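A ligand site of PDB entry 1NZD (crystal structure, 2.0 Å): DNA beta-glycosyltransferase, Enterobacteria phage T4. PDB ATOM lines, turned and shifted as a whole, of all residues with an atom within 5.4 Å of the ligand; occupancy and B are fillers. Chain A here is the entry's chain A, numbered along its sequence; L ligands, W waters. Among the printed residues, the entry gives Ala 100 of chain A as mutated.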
ATOM      1  N   PHE A  15       9.625  33.955  -9.555  1.00  0.00           N
ATOM      2  CA  PHE A  15       8.869  32.735  -9.308  1.00  0.00           C
ATOM      3  C   PHE A  15       7.441  32.965  -8.817  1.00  0.00           C
ATOM      4  O   PHE A  15       6.823  32.052  -8.270  1.00  0.00           O
ATOM      5  CB  PHE A  15       9.630  31.855  -8.307  1.00  0.00           C
ATOM      6  CG  PHE A  15      11.003  31.472  -8.786  1.00  0.00           C
ATOM      7  CD1 PHE A  15      12.086  32.321  -8.563  1.00  0.00           C
ATOM      8  CD2 PHE A  15      11.200  30.312  -9.526  1.00  0.00           C
ATOM      9  CE1 PHE A  15      13.355  32.013  -9.071  1.00  0.00           C
ATOM     10  CE2 PHE A  15      12.457  29.996 -10.035  1.00  0.00           C
ATOM     11  CZ  PHE A  15      13.530  30.847  -9.813  1.00  0.00           C
ATOM     12  N   VAL A  18       3.520  30.653 -12.457  1.00  0.00           N
ATOM     13  CA  VAL A  18       3.973  29.369 -12.942  1.00  0.00           C
ATOM     14  C   VAL A  18       4.714  29.476 -14.282  1.00  0.00           C
ATOM     15  O   VAL A  18       5.791  28.909 -14.441  1.00  0.00           O
ATOM     16  CB  VAL A  18       2.800  28.382 -13.066  1.00  0.00           C
ATOM     17  CG1 VAL A  18       3.292  27.007 -13.517  1.00  0.00           C
ATOM     18  CG2 VAL A  18       2.096  28.266 -11.712  1.00  0.00           C
ATOM     19  N   GLU A  22       8.542  28.244 -14.501  1.00  0.00           N
ATOM     20  CA  GLU A  22       8.928  27.141 -15.372  1.00  0.00           C
ATOM     21  C   GLU A  22      10.007  27.553 -16.362  1.00  0.00           C
ATOM     22  O   GLU A  22      10.962  26.810 -16.607  1.00  0.00           O
ATOM     23  CB  GLU A  22       7.698  26.607 -16.129  1.00  0.00           C
ATOM     24  CG  GLU A  22       8.005  25.505 -17.138  1.00  0.00           C
ATOM     25  CD  GLU A  22       6.803  24.611 -17.394  1.00  0.00           C
ATOM     26  OE1 GLU A  22       6.575  23.669 -16.597  1.00  0.00           O
ATOM     27  OE2 GLU A  22       6.080  24.858 -18.380  1.00  0.00           O
ATOM     28  N   THR A  99       4.168  21.427 -22.202  1.00  0.00           N
ATOM     29  CA  THR A  99       4.012  21.002 -20.817  1.00  0.00           C
ATOM     30  C   THR A  99       2.563  21.074 -20.341  1.00  0.00           C
ATOM     31  O   THR A  99       2.252  20.609 -19.243  1.00  0.00           O
ATOM     32  CB  THR A  99       4.875  21.881 -19.862  1.00  0.00           C
ATOM     33  OG1 THR A  99       4.417  23.236 -19.899  1.00  0.00           O
ATOM     34  CG2 THR A  99       6.345  21.834 -20.285  1.00  0.00           C
ATOM     35  N   ALA A 100       1.690  21.663 -21.155  1.00  0.00           N
ATOM     36  CA  ALA A 100       0.270  21.764 -20.806  1.00  0.00           C
ATOM     37  C   ALA A 100      -0.557  21.449 -22.051  1.00  0.00           C
ATOM     38  O   ALA A 100      -0.491  22.156 -23.060  1.00  0.00           O
ATOM     39  CB  ALA A 100      -0.052  23.152 -20.277  1.00  0.00           C
ATOM     40  N   ARG A 102      -3.555  21.936 -22.984  1.00  0.00           N
ATOM     41  CA  ARG A 102      -4.407  22.992 -23.519  1.00  0.00           C
ATOM     42  C   ARG A 102      -3.626  24.111 -24.238  1.00  0.00           C
ATOM     43  O   ARG A 102      -4.241  25.006 -24.811  1.00  0.00           O
ATOM     44  CB  ARG A 102      -5.230  23.614 -22.388  1.00  0.00           C
ATOM     45  CG  ARG A 102      -4.400  24.480 -21.436  1.00  0.00           C
ATOM     46  CD  ARG A 102      -5.224  25.093 -20.306  1.00  0.00           C
ATOM     47  NE  ARG A 102      -4.436  26.066 -19.538  1.00  0.00           N
ATOM     48  CZ  ARG A 102      -3.410  25.752 -18.754  1.00  0.00           C
ATOM     49  NH1 ARG A 102      -3.035  24.493 -18.602  1.00  0.00           N
ATOM     50  NH2 ARG A 102      -2.743  26.715 -18.129  1.00  0.00           N
ATOM     51  N   GLN A 137       5.725  16.525 -23.138  1.00  0.00           N
ATOM     52  CA  GLN A 137       5.953  16.061 -21.774  1.00  0.00           C
ATOM     53  C   GLN A 137       5.223  14.735 -21.606  1.00  0.00           C
ATOM     54  O   GLN A 137       5.562  13.928 -20.748  1.00  0.00           O
ATOM     55  CB  GLN A 137       5.438  17.104 -20.766  1.00  0.00           C
ATOM     56  CG  GLN A 137       5.736  16.775 -19.303  1.00  0.00           C
ATOM     57  CD  GLN A 137       5.464  17.954 -18.379  1.00  0.00           C
ATOM     58  OE1 GLN A 137       5.976  19.051 -18.603  1.00  0.00           O
ATOM     59  NE2 GLN A 137       4.647  17.731 -17.350  1.00  0.00           N
ATOM     60  N   GLU A 163       9.122  17.937 -16.980  1.00  0.00           N
ATOM     61  CA  GLU A 163       8.826  18.256 -15.588  1.00  0.00           C
ATOM     62  C   GLU A 163       9.809  17.828 -14.509  1.00  0.00           C
ATOM     63  O   GLU A 163       9.637  18.191 -13.345  1.00  0.00           O
ATOM     64  CB  GLU A 163       7.410  17.794 -15.247  1.00  0.00           C
ATOM     65  CG  GLU A 163       7.231  16.362 -14.753  1.00  0.00           C
ATOM     66  CD  GLU A 163       7.818  15.311 -15.672  1.00  0.00           C
ATOM     67  OE1 GLU A 163       7.727  15.466 -16.906  1.00  0.00           O
ATOM     68  OE2 GLU A 163       8.356  14.321 -15.149  1.00  0.00           O
ATOM     69  N   TYR A 165      12.661  18.918 -14.202  1.00  0.00           N
ATOM     70  CA  TYR A 165      13.621  19.998 -14.008  1.00  0.00           C
ATOM     71  C   TYR A 165      13.883  20.403 -12.568  1.00  0.00           C
ATOM     72  O   TYR A 165      14.992  20.803 -12.228  1.00  0.00           O
ATOM     73  CB  TYR A 165      13.259  21.228 -14.862  1.00  0.00           C
ATOM     74  CG  TYR A 165      11.889  21.835 -14.662  1.00  0.00           C
ATOM     75  CD1 TYR A 165      11.583  22.574 -13.517  1.00  0.00           C
ATOM     76  CD2 TYR A 165      10.915  21.716 -15.658  1.00  0.00           C
ATOM     77  CE1 TYR A 165      10.333  23.188 -13.374  1.00  0.00           C
ATOM     78  CE2 TYR A 165       9.666  22.331 -15.525  1.00  0.00           C
ATOM     79  CZ  TYR A 165       9.380  23.065 -14.378  1.00  0.00           C
ATOM     80  OH  TYR A 165       8.155  23.685 -14.263  1.00  0.00           O
ATOM     81  N   LYS A 166      12.897  20.282 -11.695  1.00  0.00           N
ATOM     82  CA  LYS A 166      13.133  20.643 -10.299  1.00  0.00           C
ATOM     83  C   LYS A 166      14.053  19.658  -9.565  1.00  0.00           C
ATOM     84  O   LYS A 166      14.951  20.068  -8.835  1.00  0.00           O
ATOM     85  CB  LYS A 166      11.818  20.758  -9.527  1.00  0.00           C
ATOM     86  CG  LYS A 166      11.249  22.163  -9.475  1.00  0.00           C
ATOM     87  CD  LYS A 166      10.125  22.239  -8.443  1.00  0.00           C
ATOM     88  CE  LYS A 166       9.590  23.654  -8.296  1.00  0.00           C
ATOM     89  NZ  LYS A 166       8.612  23.737  -7.169  1.00  0.00           N
ATOM     90  N   TYR A 186      -3.255  20.480  -1.280  1.00  0.00           N
ATOM     91  CA  TYR A 186      -3.159  20.491  -2.737  1.00  0.00           C
ATOM     92  C   TYR A 186      -2.885  21.921  -3.162  1.00  0.00           C
ATOM     93  O   TYR A 186      -3.638  22.833  -2.834  1.00  0.00           O
ATOM     94  CB  TYR A 186      -4.452  20.007  -3.379  1.00  0.00           C
ATOM     95  CG  TYR A 186      -4.403  19.918  -4.893  1.00  0.00           C
ATOM     96  CD1 TYR A 186      -3.860  18.794  -5.527  1.00  0.00           C
ATOM     97  CD2 TYR A 186      -4.881  20.966  -5.691  1.00  0.00           C
ATOM     98  CE1 TYR A 186      -3.808  18.721  -6.930  1.00  0.00           C
ATOM     99  CE2 TYR A 186      -4.820  20.891  -7.094  1.00  0.00           C
ATOM    100  CZ  TYR A 186      -4.290  19.769  -7.699  1.00  0.00           C
ATOM    101  OH  TYR A 186      -4.263  19.679  -9.085  1.00  0.00           O
ATOM    102  N   GLY A 187      -1.785  22.115  -3.891  1.00  0.00           N
ATOM    103  CA  GLY A 187      -1.437  23.448  -4.339  1.00  0.00           C
ATOM    104  C   GLY A 187      -1.527  23.521  -5.856  1.00  0.00           C
ATOM    105  O   GLY A 187      -0.768  22.856  -6.551  1.00  0.00           O
ATOM    106  N   GLY A 188      -2.455  24.336  -6.351  1.00  0.00           N
ATOM    107  CA  GLY A 188      -2.595  24.457  -7.791  1.00  0.00           C
ATOM    108  C   GLY A 188      -3.682  25.445  -8.180  1.00  0.00           C
ATOM    109  O   GLY A 188      -4.021  26.336  -7.408  1.00  0.00           O
ATOM    110  N   SER A 189      -4.218  25.262  -9.383  1.00  0.00           N
ATOM    111  CA  SER A 189      -5.252  26.160  -9.868  1.00  0.00           C
ATOM    112  C   SER A 189      -6.496  25.414 -10.318  1.00  0.00           C
ATOM    113  O   SER A 189      -6.480  24.191 -10.514  1.00  0.00           O
ATOM    114  CB  SER A 189      -4.703  26.996 -11.027  1.00  0.00           C
ATOM    115  OG  SER A 189      -4.263  26.164 -12.069  1.00  0.00           O
ATOM    116  N   ARG A 191      -9.371  24.193 -12.840  1.00  0.00           N
ATOM    117  CA  ARG A 191      -9.451  23.840 -14.241  1.00  0.00           C
ATOM    118  C   ARG A 191     -10.757  23.077 -14.415  1.00  0.00           C
ATOM    119  O   ARG A 191     -11.110  22.242 -13.578  1.00  0.00           O
ATOM    120  CB  ARG A 191      -8.272  22.955 -14.666  1.00  0.00           C
ATOM    121  CG  ARG A 191      -8.294  22.593 -16.151  1.00  0.00           C
ATOM    122  CD  ARG A 191      -7.204  21.579 -16.476  1.00  0.00           C
ATOM    123  NE  ARG A 191      -5.889  22.111 -16.163  1.00  0.00           N
ATOM    124  CZ  ARG A 191      -4.802  21.366 -15.982  1.00  0.00           C
ATOM    125  NH1 ARG A 191      -4.869  20.044 -16.078  1.00  0.00           N
ATOM    126  NH2 ARG A 191      -3.649  21.952 -15.685  1.00  0.00           N
ATOM    127  N   ARG A 195     -10.618  17.519 -14.168  1.00  0.00           N
ATOM    128  CA  ARG A 195      -9.822  18.018 -13.044  1.00  0.00           C
ATOM    129  C   ARG A 195     -10.760  18.596 -11.985  1.00  0.00           C
ATOM    130  O   ARG A 195     -10.578  18.362 -10.794  1.00  0.00           O
ATOM    131  CB  ARG A 195      -8.819  19.082 -13.519  1.00  0.00           C
ATOM    132  CG  ARG A 195      -8.013  19.774 -12.402  1.00  0.00           C
ATOM    133  CD  ARG A 195      -7.252  18.796 -11.503  1.00  0.00           C
ATOM    134  NE  ARG A 195      -6.323  17.942 -12.235  1.00  0.00           N
ATOM    135  CZ  ARG A 195      -5.159  18.351 -12.744  1.00  0.00           C
ATOM    136  NH1 ARG A 195      -4.754  19.600 -12.594  1.00  0.00           N
ATOM    137  NH2 ARG A 195      -4.406  17.480 -13.403  1.00  0.00           N
ATOM    138  N   PHE A 213      -4.099  25.464  -1.658  1.00  0.00           N
ATOM    139  CA  PHE A 213      -3.443  26.746  -1.894  1.00  0.00           C
ATOM    140  C   PHE A 213      -3.208  26.964  -3.385  1.00  0.00           C
ATOM    141  O   PHE A 213      -3.195  26.029  -4.171  1.00  0.00           O
ATOM    142  CB  PHE A 213      -2.128  26.872  -1.105  1.00  0.00           C
ATOM    143  CG  PHE A 213      -1.062  25.865  -1.482  1.00  0.00           C
ATOM    144  CD1 PHE A 213      -1.111  24.550  -1.013  1.00  0.00           C
ATOM    145  CD2 PHE A 213       0.032  26.257  -2.250  1.00  0.00           C
ATOM    146  CE1 PHE A 213      -0.094  23.643  -1.304  1.00  0.00           C
ATOM    147  CE2 PHE A 213       1.060  25.347  -2.550  1.00  0.00           C
ATOM    148  CZ  PHE A 213       1.000  24.034  -2.071  1.00  0.00           C
ATOM    149  N   GLY A 214      -3.034  28.230  -3.772  1.00  0.00           N
ATOM    150  CA  GLY A 214      -2.826  28.553  -5.173  1.00  0.00           C
ATOM    151  C   GLY A 214      -3.796  29.620  -5.630  1.00  0.00           C
ATOM    152  O   GLY A 214      -4.196  30.474  -4.844  1.00  0.00           O
ATOM    153  N   ASN A 215      -4.171  29.581  -6.905  1.00  0.00           N
ATOM    154  CA  ASN A 215      -5.100  30.561  -7.458  1.00  0.00           C
ATOM    155  C   ASN A 215      -6.560  30.149  -7.392  1.00  0.00           C
ATOM    156  O   ASN A 215      -7.448  30.939  -7.723  1.00  0.00           O
ATOM    157  CB  ASN A 215      -4.728  30.862  -8.904  1.00  0.00           C
ATOM    158  CG  ASN A 215      -3.419  31.594  -9.031  1.00  0.00           C
ATOM    159  OD1 ASN A 215      -3.247  32.673  -8.456  1.00  0.00           O
ATOM    160  ND2 ASN A 215      -2.483  31.016  -9.768  1.00  0.00           N
ATOM    161  N   GLY A 236      -4.098  31.757  -0.393  1.00  0.00           N
ATOM    162  CA  GLY A 236      -3.467  32.341  -1.566  1.00  0.00           C
ATOM    163  C   GLY A 236      -2.308  31.600  -2.202  1.00  0.00           C
ATOM    164  O   GLY A 236      -1.860  30.559  -1.709  1.00  0.00           O
ATOM    165  N   LYS A 237      -1.816  32.140  -3.311  1.00  0.00           N
ATOM    166  CA  LYS A 237      -0.705  31.565  -4.050  1.00  0.00           C
ATOM    167  C   LYS A 237       0.626  31.907  -3.376  1.00  0.00           C
ATOM    168  O   LYS A 237       0.723  32.862  -2.619  1.00  0.00           O
ATOM    169  CB  LYS A 237      -0.694  32.105  -5.489  1.00  0.00           C
ATOM    170  CG  LYS A 237      -0.859  33.614  -5.555  1.00  0.00           C
ATOM    171  CD  LYS A 237      -0.847  34.163  -6.983  1.00  0.00           C
ATOM    172  CE  LYS A 237       0.564  34.265  -7.531  1.00  0.00           C
ATOM    173  NZ  LYS A 237       0.616  35.156  -8.730  1.00  0.00           N
ATOM    174  N   ILE A 238       1.635  31.103  -3.666  1.00  0.00           N
ATOM    175  CA  ILE A 238       2.973  31.316  -3.134  1.00  0.00           C
ATOM    176  C   ILE A 238       3.954  31.100  -4.274  1.00  0.00           C
ATOM    177  O   ILE A 238       3.597  30.536  -5.303  1.00  0.00           O
ATOM    178  CB  ILE A 238       3.285  30.330  -1.980  1.00  0.00           C
ATOM    179  CG1 ILE A 238       3.245  28.885  -2.497  1.00  0.00           C
ATOM    180  CG2 ILE A 238       2.304  30.546  -0.841  1.00  0.00           C
ATOM    181  CD1 ILE A 238       3.760  27.863  -1.494  1.00  0.00           C
ATOM    182  N   PRO A 239       5.206  31.558  -4.109  1.00  0.00           N
ATOM    183  CA  PRO A 239       6.198  31.378  -5.177  1.00  0.00           C
ATOM    184  C   PRO A 239       6.372  29.890  -5.461  1.00  0.00           C
ATOM    185  O   PRO A 239       6.259  29.063  -4.539  1.00  0.00           O
ATOM    186  CB  PRO A 239       7.453  32.004  -4.577  1.00  0.00           C
ATOM    187  CG  PRO A 239       6.896  33.081  -3.694  1.00  0.00           C
ATOM    188  CD  PRO A 239       5.754  32.376  -3.016  1.00  0.00           C
ATOM    189  N   MET A 240       6.646  29.530  -6.715  1.00  0.00           N
ATOM    190  CA  MET A 240       6.801  28.119  -7.061  1.00  0.00           C
ATOM    191  C   MET A 240       7.948  27.434  -6.320  1.00  0.00           C
ATOM    192  O   MET A 240       7.883  26.232  -6.062  1.00  0.00           O
ATOM    193  CB  MET A 240       7.012  27.924  -8.570  1.00  0.00           C
ATOM    194  CG  MET A 240       7.162  26.433  -8.928  1.00  0.00           C
ATOM    195  SD  MET A 240       7.692  26.024 -10.588  1.00  0.00           S
ATOM    196  CE  MET A 240       6.123  26.117 -11.451  1.00  0.00           C
ATOM    197  N   VAL A 243       6.828  25.557  -2.992  1.00  0.00           N
ATOM    198  CA  VAL A 243       5.725  24.593  -3.048  1.00  0.00           C
ATOM    199  C   VAL A 243       5.950  23.331  -2.219  1.00  0.00           C
ATOM    200  O   VAL A 243       5.059  22.918  -1.471  1.00  0.00           O
ATOM    201  CB  VAL A 243       5.402  24.222  -4.524  1.00  0.00           C
ATOM    202  CG1 VAL A 243       4.456  23.032  -4.577  1.00  0.00           C
ATOM    203  CG2 VAL A 243       4.771  25.412  -5.236  1.00  0.00           C
ATOM    204  N   TYR A 261      -4.183  13.536 -19.648  1.00  0.00           N
ATOM    205  CA  TYR A 261      -2.973  13.571 -18.830  1.00  0.00           C
ATOM    206  C   TYR A 261      -2.719  12.179 -18.261  1.00  0.00           C
ATOM    207  O   TYR A 261      -1.575  11.721 -18.151  1.00  0.00           O
ATOM    208  CB  TYR A 261      -3.114  14.561 -17.665  1.00  0.00           C
ATOM    209  CG  TYR A 261      -2.814  16.003 -18.016  1.00  0.00           C
ATOM    210  CD1 TYR A 261      -3.817  16.863 -18.488  1.00  0.00           C
ATOM    211  CD2 TYR A 261      -1.525  16.525 -17.877  1.00  0.00           C
ATOM    212  CE1 TYR A 261      -3.533  18.195 -18.802  1.00  0.00           C
ATOM    213  CE2 TYR A 261      -1.235  17.845 -18.180  1.00  0.00           C
ATOM    214  CZ  TYR A 261      -2.235  18.674 -18.643  1.00  0.00           C
ATOM    215  OH  TYR A 261      -1.937  19.982 -18.946  1.00  0.00           O
ATOM    216  N   PHE A 265       1.105  11.890 -19.121  1.00  0.00           N
ATOM    217  CA  PHE A 265       1.983  12.912 -18.534  1.00  0.00           C
ATOM    218  C   PHE A 265       2.324  12.575 -17.097  1.00  0.00           C
ATOM    219  O   PHE A 265       1.559  11.913 -16.400  1.00  0.00           O
ATOM    220  CB  PHE A 265       1.267  14.265 -18.458  1.00  0.00           C
ATOM    221  CG  PHE A 265       1.399  15.139 -19.678  1.00  0.00           C
ATOM    222  CD1 PHE A 265       0.892  14.737 -20.912  1.00  0.00           C
ATOM    223  CD2 PHE A 265       1.966  16.407 -19.563  1.00  0.00           C
ATOM    224  CE1 PHE A 265       0.948  15.593 -22.020  1.00  0.00           C
ATOM    225  CE2 PHE A 265       2.031  17.261 -20.670  1.00  0.00           C
ATOM    226  CZ  PHE A 265       1.520  16.849 -21.894  1.00  0.00           C
ATOM    227  N   ILE A 266       3.490  13.042 -16.669  1.00  0.00           N
ATOM    228  CA  ILE A 266       3.871  12.974 -15.274  1.00  0.00           C
ATOM    229  C   ILE A 266       3.902  14.495 -15.119  1.00  0.00           C
ATOM    230  O   ILE A 266       4.435  15.192 -16.000  1.00  0.00           O
ATOM    231  CB  ILE A 266       5.287  12.403 -15.037  1.00  0.00           C
ATOM    232  CG1 ILE A 266       5.282  10.888 -15.230  1.00  0.00           C
ATOM    233  CG2 ILE A 266       5.743  12.748 -13.608  1.00  0.00           C
ATOM    234  CD1 ILE A 266       4.408  10.146 -14.224  1.00  0.00           C
ATOM    235  N   THR A 267       3.296  15.034 -14.068  1.00  0.00           N
ATOM    236  CA  THR A 267       3.266  16.476 -13.889  1.00  0.00           C
ATOM    237  C   THR A 267       4.261  16.915 -12.827  1.00  0.00           C
ATOM    238  O   THR A 267       4.698  16.119 -11.999  1.00  0.00           O
ATOM    239  CB  THR A 267       1.850  16.952 -13.505  1.00  0.00           C
ATOM    240  OG1 THR A 267       1.415  16.276 -12.322  1.00  0.00           O
ATOM    241  CG2 THR A 267       0.873  16.655 -14.644  1.00  0.00           C
ATOM    242  N   LEU A 268       4.640  18.197 -12.860  1.00  0.00           N
ATOM    243  CA  LEU A 268       5.593  18.771 -11.920  1.00  0.00           C
ATOM    244  C   LEU A 268       5.233  18.427 -10.474  1.00  0.00           C
ATOM    245  O   LEU A 268       6.099  18.155  -9.645  1.00  0.00           O
ATOM    246  CB  LEU A 268       5.636  20.292 -12.096  1.00  0.00           C
ATOM    247  CG  LEU A 268       6.578  21.053 -11.154  1.00  0.00           C
ATOM    248  CD1 LEU A 268       8.002  20.558 -11.357  1.00  0.00           C
ATOM    249  CD2 LEU A 268       6.492  22.553 -11.423  1.00  0.00           C
ATOM    250  N   ARG A 269       3.930  18.465 -10.205  1.00  0.00           N
ATOM    251  CA  ARG A 269       3.348  18.173  -8.901  1.00  0.00           C
ATOM    252  C   ARG A 269       3.820  16.847  -8.318  1.00  0.00           C
ATOM    253  O   ARG A 269       4.054  16.725  -7.110  1.00  0.00           O
ATOM    254  CB  ARG A 269       1.824  18.180  -9.057  1.00  0.00           C
ATOM    255  CG  ARG A 269       1.013  17.655  -7.900  1.00  0.00           C
ATOM    256  CD  ARG A 269      -0.458  17.650  -8.312  1.00  0.00           C
ATOM    257  NE  ARG A 269      -0.832  18.945  -8.905  1.00  0.00           N
ATOM    258  CZ  ARG A 269      -0.830  20.086  -8.235  1.00  0.00           C
ATOM    259  NH1 ARG A 269      -0.481  20.111  -6.943  1.00  0.00           N
ATOM    260  NH2 ARG A 269      -1.144  21.226  -8.844  1.00  0.00           N
ATOM    261  N   GLU A 272       7.172  17.444  -6.872  1.00  0.00           N
ATOM    262  CA  GLU A 272       7.076  18.385  -5.742  1.00  0.00           C
ATOM    263  C   GLU A 272       6.498  17.686  -4.524  1.00  0.00           C
ATOM    264  O   GLU A 272       6.868  17.977  -3.387  1.00  0.00           O
ATOM    265  CB  GLU A 272       6.182  19.567  -6.109  1.00  0.00           C
ATOM    266  CG  GLU A 272       6.651  20.390  -7.306  1.00  0.00           C
ATOM    267  CD  GLU A 272       5.690  21.513  -7.639  1.00  0.00           C
ATOM    268  OE1 GLU A 272       4.483  21.219  -7.807  1.00  0.00           O
ATOM    269  OE2 GLU A 272       6.123  22.683  -7.740  1.00  0.00           O
HETATM  270  N1  LIG L   1       1.967  26.466  -7.739  1.00  0.00           N
HETATM  271  C1  LIG L   1       2.584  27.630  -7.328  1.00  0.00           C
HETATM  272  N2  LIG L   1       1.978  28.262  -6.285  1.00  0.00           N
HETATM  273  C2  LIG L   1       0.834  27.875  -5.623  1.00  0.00           C
HETATM  274  C3  LIG L   1       0.245  26.666  -6.113  1.00  0.00           C
HETATM  275  C4  LIG L   1       0.816  26.021  -7.139  1.00  0.00           C
HETATM  276  O1  LIG L   1       3.601  28.060  -7.851  1.00  0.00           O
HETATM  277  O2  LIG L   1       0.407  28.565  -4.702  1.00  0.00           O
HETATM  278  C5  LIG L   1       2.607  25.727  -8.840  1.00  0.00           C
HETATM  279  C6  LIG L   1       3.190  24.354  -8.448  1.00  0.00           C
HETATM  280  O3  LIG L   1       4.558  24.336  -8.811  1.00  0.00           O
HETATM  281  C7  LIG L   1       2.315  23.390  -9.255  1.00  0.00           C
HETATM  282  C8  LIG L   1       1.999  24.226 -10.492  1.00  0.00           C
HETATM  283  O4  LIG L   1       1.700  25.514  -9.891  1.00  0.00           O
HETATM  284  O5  LIG L   1       3.037  22.220  -9.620  1.00  0.00           O
HETATM  285  C9  LIG L   1       0.897  23.774 -11.425  1.00  0.00           C
HETATM  286  O6  LIG L   1      -0.307  23.561 -10.717  1.00  0.00           O
HETATM  287  P1  LIG L   1      -1.701  23.604 -11.492  1.00  0.00           P
HETATM  288  O7  LIG L   1      -2.743  22.964 -10.642  1.00  0.00           O
HETATM  289  O8  LIG L   1      -1.914  24.975 -11.997  1.00  0.00           O
HETATM  290  O9  LIG L   1      -1.442  22.666 -12.795  1.00  0.00           O
HETATM  291  P2  LIG L   1      -1.110  21.078 -12.925  1.00  0.00           P
HETATM  292  O10 LIG L   1      -2.186  20.463 -13.747  1.00  0.00           O
HETATM  293  O11 LIG L   1      -0.795  20.525 -11.583  1.00  0.00           O
HETATM  294  O12 LIG L   1       0.228  21.074 -13.783  1.00  0.00           O
HETATM  295  C10 LIG L   1       0.396  21.847 -14.962  1.00  0.00           C
HETATM  296  C11 LIG L   1       0.569  20.975 -16.193  1.00  0.00           C
HETATM  297  C12 LIG L   1       1.740  20.036 -15.925  1.00  0.00           C
HETATM  298  C13 LIG L   1       3.006  20.855 -15.644  1.00  0.00           C
HETATM  299  C14 LIG L   1       2.771  21.876 -14.507  1.00  0.00           C
HETATM  300  C15 LIG L   1       3.916  22.860 -14.417  1.00  0.00           C
HETATM  301  O13 LIG L   1      -0.625  20.241 -16.395  1.00  0.00           O
HETATM  302  O14 LIG L   1       1.949  19.194 -17.042  1.00  0.00           O
HETATM  303  O15 LIG L   1       4.068  19.986 -15.276  1.00  0.00           O
HETATM  304  O16 LIG L   1       1.575  22.656 -14.759  1.00  0.00           O
HETATM  305  O17 LIG L   1       4.007  23.650 -15.603  1.00  0.00           O
HETATM  306  O   HOH W   1      -5.042  21.698 -10.684  1.00  0.00           O
HETATM  307  O   HOH W   2      -0.935  17.670 -11.839  1.00  0.00           O
HETATM  308  O   HOH W   3       6.308  20.920 -16.492  1.00  0.00           O
HETATM  309  O   HOH W   4      -0.516  27.188 -13.160  1.00  0.00           O
HETATM  310  O   HOH W   5      -1.804  25.650 -14.660  1.00  0.00           O
HETATM  311  O   HOH W   6       4.012  30.866  -8.674  1.00  0.00           O
HETATM  312  O   HOH W   7      -2.533  18.323 -15.351  1.00  0.00           O
HETATM  313  O   HOH W   8       2.038  20.203 -11.429  1.00  0.00           O
HETATM  314  O   HOH W   9      -1.076  26.798 -10.116  1.00  0.00           O
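An oxygen (O3) of the ligand lies within hydrogen-bond range of the side-chain carboxylate (OE2) of Glu 272 (2.5 Å).
The backbone NH of Ser 189 sits at hydrogen-bond distance from an oxygen (O7) of the ligand, at 3.0 Å.
The side-chain hydroxyl (OG) of Ser 189 sits at hydrogen-bond distance from an oxygen (O8) of the ligand (2.6 Å).
O14 of the ligand sits at hydrogen-bond distance from O of Thr 99 (2.6 Å).
The side-chain carboxylate (OE1) of Glu 22 sits at hydrogen-bond distance from an oxygen (O17) of the ligand (2.8 Å).
O10 of the ligand lies within salt-bridge range of NH2 of Arg 191.
The guanidinium group (NH2) of Arg 269 is in salt-bridge range of an oxygen (O11) of the ligand (2.8 Å).
An oxygen (O13) of the ligand lies within hydrogen-bond range of the side-chain hydroxyl of Tyr 261, at 2.9 Å.
O10 of the ligand lies within salt-bridge range of NH1 of Arg 195 (2.9 Å).
An oxygen (O2) of the ligand is in hydrogen-bond range of the backbone NH of Ile 238, at 3.0 Å.
The backbone carbonyl oxygen of Ile 238 lies within hydrogen-bond range of a nitrogen (N2) of the ligand (3.0 Å).
The backbone NH of Leu 268 lies within hydrogen-bond range of an oxygen (O15) of the ligand, at 3.1 Å.
The side-chain amide nitrogen of Gln 137 is in hydrogen-bond range of an oxygen (O14) of the ligand, 3.1 Å away.
OE2 of Glu 272 lies within salt-bridge range of NZ of Lys 166, 2.8 Å away.
The side-chain hydroxyl of Thr 99 is in hydrogen-bond range of the side-chain carboxylate of Glu 22 (2.8 Å).
The side-chain carboxylate (OE1) of Glu 22 lies within hydrogen-bond range of the side-chain hydroxyl (OH) of Tyr 165 (2.8 Å).
NH1 of Arg 269 lies within hydrogen-bond range of O of Gly 187 (2.8 Å).
NH2 of Arg 269 is in hydrogen-bond range of OH of Tyr 186.
The backbone NH (N) of Gly 188 is in hydrogen-bond range of the backbone carbonyl oxygen (O) of Phe 213, at 2.9 Å.
The backbone carbonyl oxygen of Gly 188 sits at hydrogen-bond distance from the backbone NH of Asn 215 (3.3 Å).
The backbone carbonyl oxygen (O) of Tyr 186 sits at hydrogen-bond distance from the backbone NH (N) of Phe 213, at 2.9 Å.
Residues that only touch the ligand: Val 18 (3.3 Å), Glu 163 (3.997 Å), Tyr 186 (3.9 Å), Gly 187 (3.6 Å), Gly 188 (3.2 Å), Phe 213 (3.4 Å), Gly 214 (3.3 Å), Lys 237 (3.3 Å), Met 240 (3.3 Å), Val 243 (3.7 Å), Phe 265 (3.8 Å) and Thr 267 (3.7 Å).
Water W1 lies within hydrogen-bond range of an oxygen (O7) of the ligand (2.6 Å), the side-chain hydroxyl (OH) of Tyr 186 (2.7 Å), the guanidinium group (NH1) of Arg 195 (2.9 Å) and the backbone carbonyl oxygen (O) of Ser 189 (2.9 Å).
Water W7 lies within hydrogen-bond range of O10 of the ligand (2.7 Å), NH2 of Arg 195 (2.8 Å) and NH1 of Arg 191 (3.0 Å).
Water W3 lies within hydrogen-bond range of an oxygen (O15) of the ligand (2.7 Å), the side-chain carboxylate (OE1) of Glu 22 (2.8 Å) and the side-chain amide oxygen (OE1) of Gln 137 (2.8 Å).
Water W8 bridges N of Arg 269 (2.8 Å) and O11 of the ligand (2.9 Å).
Water W2 lies within hydrogen-bond range of OG1 of Thr 267 (2.8 Å), O11 of the ligand (2.9 Å) and NE of Arg 269 (3.2 Å).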
